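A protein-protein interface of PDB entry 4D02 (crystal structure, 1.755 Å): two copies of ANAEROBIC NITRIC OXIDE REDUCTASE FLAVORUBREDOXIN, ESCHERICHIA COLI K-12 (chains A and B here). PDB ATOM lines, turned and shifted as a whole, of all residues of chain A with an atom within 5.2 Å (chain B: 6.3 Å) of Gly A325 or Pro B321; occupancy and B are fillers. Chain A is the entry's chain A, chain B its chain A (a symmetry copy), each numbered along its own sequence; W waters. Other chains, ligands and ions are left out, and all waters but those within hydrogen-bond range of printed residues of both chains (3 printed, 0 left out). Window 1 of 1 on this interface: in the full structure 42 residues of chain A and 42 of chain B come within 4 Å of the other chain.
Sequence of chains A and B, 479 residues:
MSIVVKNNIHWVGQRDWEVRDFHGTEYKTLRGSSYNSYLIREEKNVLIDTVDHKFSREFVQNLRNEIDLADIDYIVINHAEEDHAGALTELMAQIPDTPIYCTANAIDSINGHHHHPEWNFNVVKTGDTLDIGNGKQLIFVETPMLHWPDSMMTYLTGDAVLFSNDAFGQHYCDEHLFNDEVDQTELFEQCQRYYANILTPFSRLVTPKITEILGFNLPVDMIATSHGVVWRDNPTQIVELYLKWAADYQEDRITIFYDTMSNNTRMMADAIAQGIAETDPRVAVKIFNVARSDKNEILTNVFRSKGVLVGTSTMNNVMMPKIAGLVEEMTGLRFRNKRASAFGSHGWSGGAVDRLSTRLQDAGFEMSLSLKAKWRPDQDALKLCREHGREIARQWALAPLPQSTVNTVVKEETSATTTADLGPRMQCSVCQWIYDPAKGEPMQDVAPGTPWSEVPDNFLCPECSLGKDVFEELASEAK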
ATOM      1  N   GLU A  26     -29.982  -3.271  24.859  1.00  0.00           N
ATOM      2  CA  GLU A  26     -28.980  -4.334  24.698  1.00  0.00           C
ATOM      3  C   GLU A  26     -28.500  -4.940  26.011  1.00  0.00           C
ATOM      4  O   GLU A  26     -28.000  -6.064  26.025  1.00  0.00           O
ATOM      5  CB  GLU A  26     -27.765  -3.821  23.918  1.00  0.00           C
ATOM      6  CG  GLU A  26     -28.085  -3.401  22.495  1.00  0.00           C
ATOM      7  CD  GLU A  26     -28.963  -4.402  21.778  1.00  0.00           C
ATOM      8  OE1 GLU A  26     -28.734  -5.622  21.924  1.00  0.00           O
ATOM      9  OE2 GLU A  26     -29.892  -3.973  21.067  1.00  0.00           O
ATOM     10  N   LYS A 295     -31.966 -12.235  26.698  1.00  0.00           N
ATOM     11  CA  LYS A 295     -30.801 -12.289  25.823  1.00  0.00           C
ATOM     12  C   LYS A 295     -29.481 -12.236  26.597  1.00  0.00           C
ATOM     13  O   LYS A 295     -28.527 -12.968  26.300  1.00  0.00           O
ATOM     14  CB  LYS A 295     -30.868 -11.131  24.820  1.00  0.00           C
ATOM     15  CG  LYS A 295     -29.715 -11.087  23.863  1.00  0.00           C
ATOM     16  CD  LYS A 295     -29.507  -9.688  23.315  1.00  0.00           C
ATOM     17  CE  LYS A 295     -28.807  -8.810  24.318  1.00  0.00           C
ATOM     18  NZ  LYS A 295     -28.142  -7.654  23.660  1.00  0.00           N
ATOM     19  N   PRO A 321     -34.591 -14.420  12.242  1.00  0.00           N
ATOM     20  CA  PRO A 321     -33.937 -13.124  12.469  1.00  0.00           C
ATOM     21  C   PRO A 321     -33.323 -12.957  13.859  1.00  0.00           C
ATOM     22  O   PRO A 321     -32.260 -12.344  13.957  1.00  0.00           O
ATOM     23  CB  PRO A 321     -35.075 -12.105  12.250  1.00  0.00           C
ATOM     24  CG  PRO A 321     -36.339 -12.887  12.328  1.00  0.00           C
ATOM     25  CD  PRO A 321     -36.006 -14.266  11.853  1.00  0.00           C
ATOM     26  N   LYS A 322     -33.947 -13.480  14.909  1.00  0.00           N
ATOM     27  CA  LYS A 322     -33.376 -13.290  16.244  1.00  0.00           C
ATOM     28  C   LYS A 322     -32.073 -14.058  16.377  1.00  0.00           C
ATOM     29  O   LYS A 322     -31.183 -13.667  17.139  1.00  0.00           O
ATOM     30  CB  LYS A 322     -34.348 -13.723  17.342  1.00  0.00           C
ATOM     31  CG  LYS A 322     -35.639 -12.904  17.386  1.00  0.00           C
ATOM     32  CD  LYS A 322     -36.436 -13.229  18.639  1.00  0.00           C
ATOM     33  CE  LYS A 322     -37.905 -12.980  18.409  1.00  0.00           C
ATOM     34  NZ  LYS A 322     -38.416 -13.881  17.338  1.00  0.00           N
ATOM     35  N   ILE A 323     -31.955 -15.159  15.640  1.00  0.00           N
ATOM     36  CA  ILE A 323     -30.714 -15.926  15.646  1.00  0.00           C
ATOM     37  C   ILE A 323     -29.637 -15.154  14.869  1.00  0.00           C
ATOM     38  O   ILE A 323     -28.495 -15.047  15.319  1.00  0.00           O
ATOM     39  CB  ILE A 323     -30.920 -17.344  15.056  1.00  0.00           C
ATOM     40  CG1 ILE A 323     -31.874 -18.159  15.944  1.00  0.00           C
ATOM     41  CG2 ILE A 323     -29.582 -18.083  14.904  1.00  0.00           C
ATOM     42  CD1 ILE A 323     -31.327 -18.482  17.325  1.00  0.00           C
ATOM     43  N   ALA A 324     -30.003 -14.600  13.715  1.00  0.00           N
ATOM     44  CA  ALA A 324     -29.065 -13.773  12.957  1.00  0.00           C
ATOM     45  C   ALA A 324     -28.568 -12.597  13.806  1.00  0.00           C
ATOM     46  O   ALA A 324     -27.372 -12.281  13.820  1.00  0.00           O
ATOM     47  CB  ALA A 324     -29.713 -13.273  11.674  1.00  0.00           C
ATOM     48  N   GLY A 325     -29.488 -11.964  14.528  1.00  0.00           N
ATOM     49  CA  GLY A 325     -29.130 -10.870  15.410  1.00  0.00           C
ATOM     50  C   GLY A 325     -28.170 -11.294  16.510  1.00  0.00           C
ATOM     51  O   GLY A 325     -27.184 -10.613  16.792  1.00  0.00           O
ATOM     52  N   LEU A 326     -28.453 -12.429  17.135  1.00  0.00           N
ATOM     53  CA  LEU A 326     -27.602 -12.921  18.210  1.00  0.00           C
ATOM     54  C   LEU A 326     -26.217 -13.293  17.680  1.00  0.00           C
ATOM     55  O   LEU A 326     -25.206 -13.087  18.348  1.00  0.00           O
ATOM     56  CB  LEU A 326     -28.264 -14.117  18.891  1.00  0.00           C
ATOM     57  CG  LEU A 326     -27.997 -14.421  20.365  1.00  0.00           C
ATOM     58  CD1 LEU A 326     -27.651 -13.191  21.192  1.00  0.00           C
ATOM     59  CD2 LEU A 326     -29.231 -15.084  20.908  1.00  0.00           C
ATOM     60  N   VAL A 327     -26.169 -13.830  16.466  1.00  0.00           N
ATOM     61  CA  VAL A 327     -24.888 -14.214  15.880  1.00  0.00           C
ATOM     62  C   VAL A 327     -24.087 -12.962  15.544  1.00  0.00           C
ATOM     63  O   VAL A 327     -22.869 -12.932  15.723  1.00  0.00           O
ATOM     64  CB  VAL A 327     -25.076 -15.099  14.625  1.00  0.00           C
ATOM     65  CG1 VAL A 327     -23.795 -15.174  13.797  1.00  0.00           C
ATOM     66  CG2 VAL A 327     -25.532 -16.496  15.042  1.00  0.00           C
ATOM     67  N   GLU A 328     -24.768 -11.919  15.077  1.00  0.00           N
ATOM     68  CA  GLU A 328     -24.095 -10.646  14.852  1.00  0.00           C
ATOM     69  C   GLU A 328     -23.474 -10.166  16.164  1.00  0.00           C
ATOM     70  O   GLU A 328     -22.293  -9.808  16.209  1.00  0.00           O
ATOM     71  CB  GLU A 328     -25.062  -9.592  14.304  1.00  0.00           C
ATOM     72  CG  GLU A 328     -24.435  -8.199  14.108  1.00  0.00           C
ATOM     73  CD  GLU A 328     -23.658  -8.042  12.797  1.00  0.00           C
ATOM     74  OE1 GLU A 328     -23.400  -9.052  12.100  1.00  0.00           O
ATOM     75  OE2 GLU A 328     -23.306  -6.890  12.456  1.00  0.00           O
ATOM     76  N   GLU A 329     -24.256 -10.175  17.237  1.00  0.00           N
ATOM     77  CA  GLU A 329     -23.749  -9.657  18.501  1.00  0.00           C
ATOM     78  C   GLU A 329     -22.576 -10.487  19.003  1.00  0.00           C
ATOM     79  O   GLU A 329     -21.590  -9.937  19.496  1.00  0.00           O
ATOM     80  CB  GLU A 329     -24.836  -9.606  19.579  1.00  0.00           C
ATOM     81  CG  GLU A 329     -24.296  -8.978  20.855  1.00  0.00           C
ATOM     82  CD  GLU A 329     -25.360  -8.658  21.874  1.00  0.00           C
ATOM     83  OE1 GLU A 329     -26.543  -8.999  21.646  1.00  0.00           O
ATOM     84  OE2 GLU A 329     -24.999  -8.064  22.913  1.00  0.00           O
ATOM     85  N   MET A 330     -22.687 -11.807  18.880  1.00  0.00           N
ATOM     86  CA  MET A 330     -21.607 -12.694  19.314  1.00  0.00           C
ATOM     87  C   MET A 330     -20.326 -12.443  18.520  1.00  0.00           C
ATOM     88  O   MET A 330     -19.224 -12.543  19.061  1.00  0.00           O
ATOM     89  CB  MET A 330     -22.032 -14.156  19.189  1.00  0.00           C
ATOM     90  CG  MET A 330     -23.107 -14.549  20.186  1.00  0.00           C
ATOM     91  SD  MET A 330     -23.305 -16.333  20.263  1.00  0.00           S
ATOM     92  CE  MET A 330     -24.078 -16.625  18.688  1.00  0.00           C
ATOM     93  N   ASP B 259     -31.844   1.362  15.388  1.00  0.00           N
ATOM     94  CA  ASP B 259     -31.701   1.121  16.816  1.00  0.00           C
ATOM     95  C   ASP B 259     -30.613   2.083  17.277  1.00  0.00           C
ATOM     96  O   ASP B 259     -29.887   2.651  16.453  1.00  0.00           O
ATOM     97  CB  ASP B 259     -31.352  -0.339  17.124  1.00  0.00           C
ATOM     98  CG  ASP B 259     -31.801  -0.777  18.524  1.00  0.00           C
ATOM     99  OD1 ASP B 259     -31.977   0.085  19.411  1.00  0.00           O
ATOM    100  OD2 ASP B 259     -31.971  -1.995  18.738  1.00  0.00           O
ATOM    101  N   THR B 312     -28.060   2.525  12.376  1.00  0.00           N
ATOM    102  CA  THR B 312     -27.412   1.777  13.439  1.00  0.00           C
ATOM    103  C   THR B 312     -26.167   2.535  13.853  1.00  0.00           C
ATOM    104  O   THR B 312     -25.524   3.179  13.027  1.00  0.00           O
ATOM    105  CB  THR B 312     -27.020   0.343  13.008  1.00  0.00           C
ATOM    106  OG1 THR B 312     -26.416  -0.349  14.115  1.00  0.00           O
ATOM    107  CG2 THR B 312     -26.025   0.372  11.850  1.00  0.00           C
ATOM    108  N   MET B 315     -21.364  -1.018  17.292  1.00  0.00           N
ATOM    109  CA  MET B 315     -21.320  -1.683  18.583  1.00  0.00           C
ATOM    110  C   MET B 315     -20.370  -2.872  18.492  1.00  0.00           C
ATOM    111  O   MET B 315     -20.682  -3.867  17.840  1.00  0.00           O
ATOM    112  CB  MET B 315     -22.727  -2.130  18.986  1.00  0.00           C
ATOM    113  CG  MET B 315     -22.819  -2.924  20.285  1.00  0.00           C
ATOM    114  SD  MET B 315     -24.487  -3.605  20.487  1.00  0.00           S
ATOM    115  CE  MET B 315     -24.376  -4.351  22.111  1.00  0.00           C
ATOM    116  N   MET B 319     -22.871  -4.107  13.662  1.00  0.00           N
ATOM    117  CA  MET B 319     -24.069  -3.293  13.766  1.00  0.00           C
ATOM    118  C   MET B 319     -24.874  -3.782  14.954  1.00  0.00           C
ATOM    119  O   MET B 319     -24.575  -4.831  15.529  1.00  0.00           O
ATOM    120  CB  MET B 319     -24.895  -3.327  12.472  1.00  0.00           C
ATOM    121  CG  MET B 319     -25.663  -4.607  12.187  1.00  0.00           C
ATOM    122  SD  MET B 319     -26.311  -4.609  10.481  1.00  0.00           S
ATOM    123  CE  MET B 319     -24.811  -4.449   9.581  1.00  0.00           C
ATOM    124  N   MET B 320     -25.874  -3.009  15.348  1.00  0.00           N
ATOM    125  CA  MET B 320     -26.707  -3.425  16.462  1.00  0.00           C
ATOM    126  C   MET B 320     -27.521  -4.650  16.043  1.00  0.00           C
ATOM    127  O   MET B 320     -27.984  -4.737  14.903  1.00  0.00           O
ATOM    128  CB  MET B 320     -27.580  -2.267  16.924  1.00  0.00           C
ATOM    129  CG  MET B 320     -26.748  -1.173  17.596  1.00  0.00           C
ATOM    130  SD  MET B 320     -27.743   0.138  18.329  1.00  0.00           S
ATOM    131  CE  MET B 320     -28.442  -0.704  19.771  1.00  0.00           C
ATOM    132  N   PRO B 321     -27.653  -5.627  16.956  1.00  0.00           N
ATOM    133  CA  PRO B 321     -28.197  -6.948  16.615  1.00  0.00           C
ATOM    134  C   PRO B 321     -29.625  -6.926  16.071  1.00  0.00           C
ATOM    135  O   PRO B 321     -29.920  -7.716  15.175  1.00  0.00           O
ATOM    136  CB  PRO B 321     -28.137  -7.716  17.952  1.00  0.00           C
ATOM    137  CG  PRO B 321     -27.964  -6.680  19.006  1.00  0.00           C
ATOM    138  CD  PRO B 321     -27.220  -5.551  18.364  1.00  0.00           C
ATOM    139  N   LYS B 322     -30.495  -6.054  16.571  1.00  0.00           N
ATOM    140  CA  LYS B 322     -31.872  -6.058  16.071  1.00  0.00           C
ATOM    141  C   LYS B 322     -31.914  -5.582  14.631  1.00  0.00           C
ATOM    142  O   LYS B 322     -32.796  -5.976  13.861  1.00  0.00           O
ATOM    143  CB  LYS B 322     -32.787  -5.186  16.933  1.00  0.00           C
ATOM    144  CG  LYS B 322     -32.929  -5.671  18.377  1.00  0.00           C
ATOM    145  CD  LYS B 322     -34.030  -4.905  19.092  1.00  0.00           C
ATOM    146  CE  LYS B 322     -33.769  -4.873  20.577  1.00  0.00           C
ATOM    147  NZ  LYS B 322     -32.497  -4.148  20.859  1.00  0.00           N
ATOM    148  N   ILE B 323     -30.963  -4.730  14.258  1.00  0.00           N
ATOM    149  CA  ILE B 323     -30.878  -4.271  12.876  1.00  0.00           C
ATOM    150  C   ILE B 323     -30.356  -5.415  11.993  1.00  0.00           C
ATOM    151  O   ILE B 323     -30.888  -5.664  10.911  1.00  0.00           O
ATOM    152  CB  ILE B 323     -29.981  -3.014  12.750  1.00  0.00           C
ATOM    153  CG1 ILE B 323     -30.610  -1.832  13.503  1.00  0.00           C
ATOM    154  CG2 ILE B 323     -29.755  -2.639  11.276  1.00  0.00           C
ATOM    155  CD1 ILE B 323     -31.918  -1.331  12.913  1.00  0.00           C
ATOM    156  N   ALA B 324     -29.330  -6.123  12.463  1.00  0.00           N
ATOM    157  CA  ALA B 324     -28.831  -7.284  11.729  1.00  0.00           C
ATOM    158  C   ALA B 324     -29.945  -8.317  11.521  1.00  0.00           C
ATOM    159  O   ALA B 324     -30.101  -8.875  10.428  1.00  0.00           O
ATOM    160  CB  ALA B 324     -27.650  -7.909  12.459  1.00  0.00           C
ATOM    161  N   GLY B 325     -30.729  -8.553  12.567  1.00  0.00           N
ATOM    162  CA  GLY B 325     -31.850  -9.470  12.476  1.00  0.00           C
ATOM    163  C   GLY B 325     -32.888  -9.028  11.457  1.00  0.00           C
ATOM    164  O   GLY B 325     -33.372  -9.826  10.655  1.00  0.00           O
ATOM    165  N   LEU B 326     -33.231  -7.747  11.482  1.00  0.00           N
ATOM    166  CA  LEU B 326     -34.223  -7.223  10.554  1.00  0.00           C
ATOM    167  C   LEU B 326     -33.710  -7.292   9.115  1.00  0.00           C
ATOM    168  O   LEU B 326     -34.469  -7.556   8.184  1.00  0.00           O
ATOM    169  CB  LEU B 326     -34.585  -5.788  10.935  1.00  0.00           C
ATOM    170  CG  LEU B 326     -35.970  -5.224  10.622  1.00  0.00           C
ATOM    171  CD1 LEU B 326     -37.066  -6.280  10.573  1.00  0.00           C
ATOM    172  CD2 LEU B 326     -36.278  -4.202  11.679  1.00  0.00           C
ATOM    173  N   GLU B 328     -31.565  -9.502   7.987  1.00  0.00           N
ATOM    174  CA  GLU B 328     -31.666 -10.908   7.617  1.00  0.00           C
ATOM    175  C   GLU B 328     -33.086 -11.202   7.135  1.00  0.00           C
ATOM    176  O   GLU B 328     -33.281 -11.790   6.066  1.00  0.00           O
ATOM    177  CB  GLU B 328     -31.302 -11.821   8.792  1.00  0.00           C
ATOM    178  CG  GLU B 328     -31.454 -13.326   8.494  1.00  0.00           C
ATOM    179  CD  GLU B 328     -30.259 -13.941   7.759  1.00  0.00           C
ATOM    180  OE1 GLU B 328     -29.376 -13.196   7.272  1.00  0.00           O
ATOM    181  OE2 GLU B 328     -30.200 -15.188   7.673  1.00  0.00           O
HETATM  182  O   HOH W   1     -31.295  -1.684  21.666  1.00  0.00           O
HETATM  183  O   HOH W   2     -30.041  -3.862  18.495  1.00  0.00           O
HETATM  184  O   HOH W   3     -30.943  -6.464  21.147  1.00  0.00           O
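NZ of Lys B322 is in salt-bridge range of OE2 of Glu A26.
The backbone NH (N) of Met B319 lies within hydrogen-bond range of the side-chain carboxylate (OE2) of Glu A328 (3.1 Å).
The side-chain amino group of Lys A295 is in salt-bridge range of the side-chain carboxylate of Glu A26 (2.7 Å).
The side-chain amino group (NZ) of Lys A295 is in salt-bridge range of the side-chain carboxylate (OE1) of Glu A329 (2.9 Å).
NZ of Lys B322 lies within salt-bridge range of OD2 of Asp B259 (3.1 Å).
N of Met B320 is in hydrogen-bond range of OG1 of Thr B312 (3.0 Å).
Glu A26 touches Asp B259 (OE2 to OD2, 3.7 Å).
Met B315 touches Glu A26 (CE to CG, 3.8 Å).
Glu A26 touches Met B320.
Glu A26 touches Pro B321.
Pro A321 touches Gly B325.
Ala A324 touches Glu B328.
Gly A325 touches Pro B321.
Glu A328 touches Ala B324 (CB to CB, 3.6 Å).
Met B315 touches Glu A329.
Pro B321 touches Glu A329 (CG to OE1, 3.8 Å).
Of the printed residues of chain B, Pro A321 touches Gly B325 (3.3 Å).
Printed residues of chain B within 4 Å of Ala A324: Glu B328.
Of the printed residues of chain B, Gly A325 touches Pro B321 (3.3 Å).
Of the printed residues of chain B, Glu A329 touches Met B315 (3.8 Å) and Pro B321 (3.8 Å).
Thr B312 touches none of the printed residues of chain A.
Pro B321 touches just these residues of chain A: Glu A26 (3.2 Å), Gly A325 (3.3 Å) and Glu A329 (3.8 Å).
Of the printed residues of chain A, Glu B328 touches Ala A324 (3.6 Å).
The nearest printed residue of chain B that does not touch Gly A325 is Gly B325 (4.001 Å).
Hydrophobic or aromatic side chains of chain A within 4 Å of the printed part of chain B: Pro A321 and Ala A324.
Hydrophobic or aromatic side chains of chain B that line the printed part of chain A: Met B315, Met B319, Met B320, Pro B321 and Ala B324.
Among the printed residues, Asp or Glu carboxylates within 4 Å of a Lys or Arg side-chain nitrogen of the other chain: Glu A26 with Lys B322 (2.6 Å).
Pro A321 touches Gly B325, and with the chains exchanged Gly A325 touches Pro B321.
Ala A324 touches Glu B328, and with the chains exchanged Glu A328 touches Ala B324.
Positions printed for both chains: 321, 322, 323, 324, 325, 326 and 328.
Of the 12 pairs that touch across the chains among the printed residues, 4 have their exchanged pair printed and touching as well.
Water W3 lies within hydrogen-bond range of the side-chain carboxylate of Glu A26 and the side-chain amino group of Lys B322.
Water W2 lies within hydrogen-bond range of the side-chain carboxylate of Glu A26, the side-chain carboxylate of Asp B259 and the backbone NH of Lys B322.
Water W1 lies within hydrogen-bond range of the side-chain carboxylate (OE2) of Glu A26 (2.8 Å), the side-chain amino group (NZ) of Lys B322 (2.9 Å) and the side-chain carboxylate (OD1) of Asp B259 (2.9 Å).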
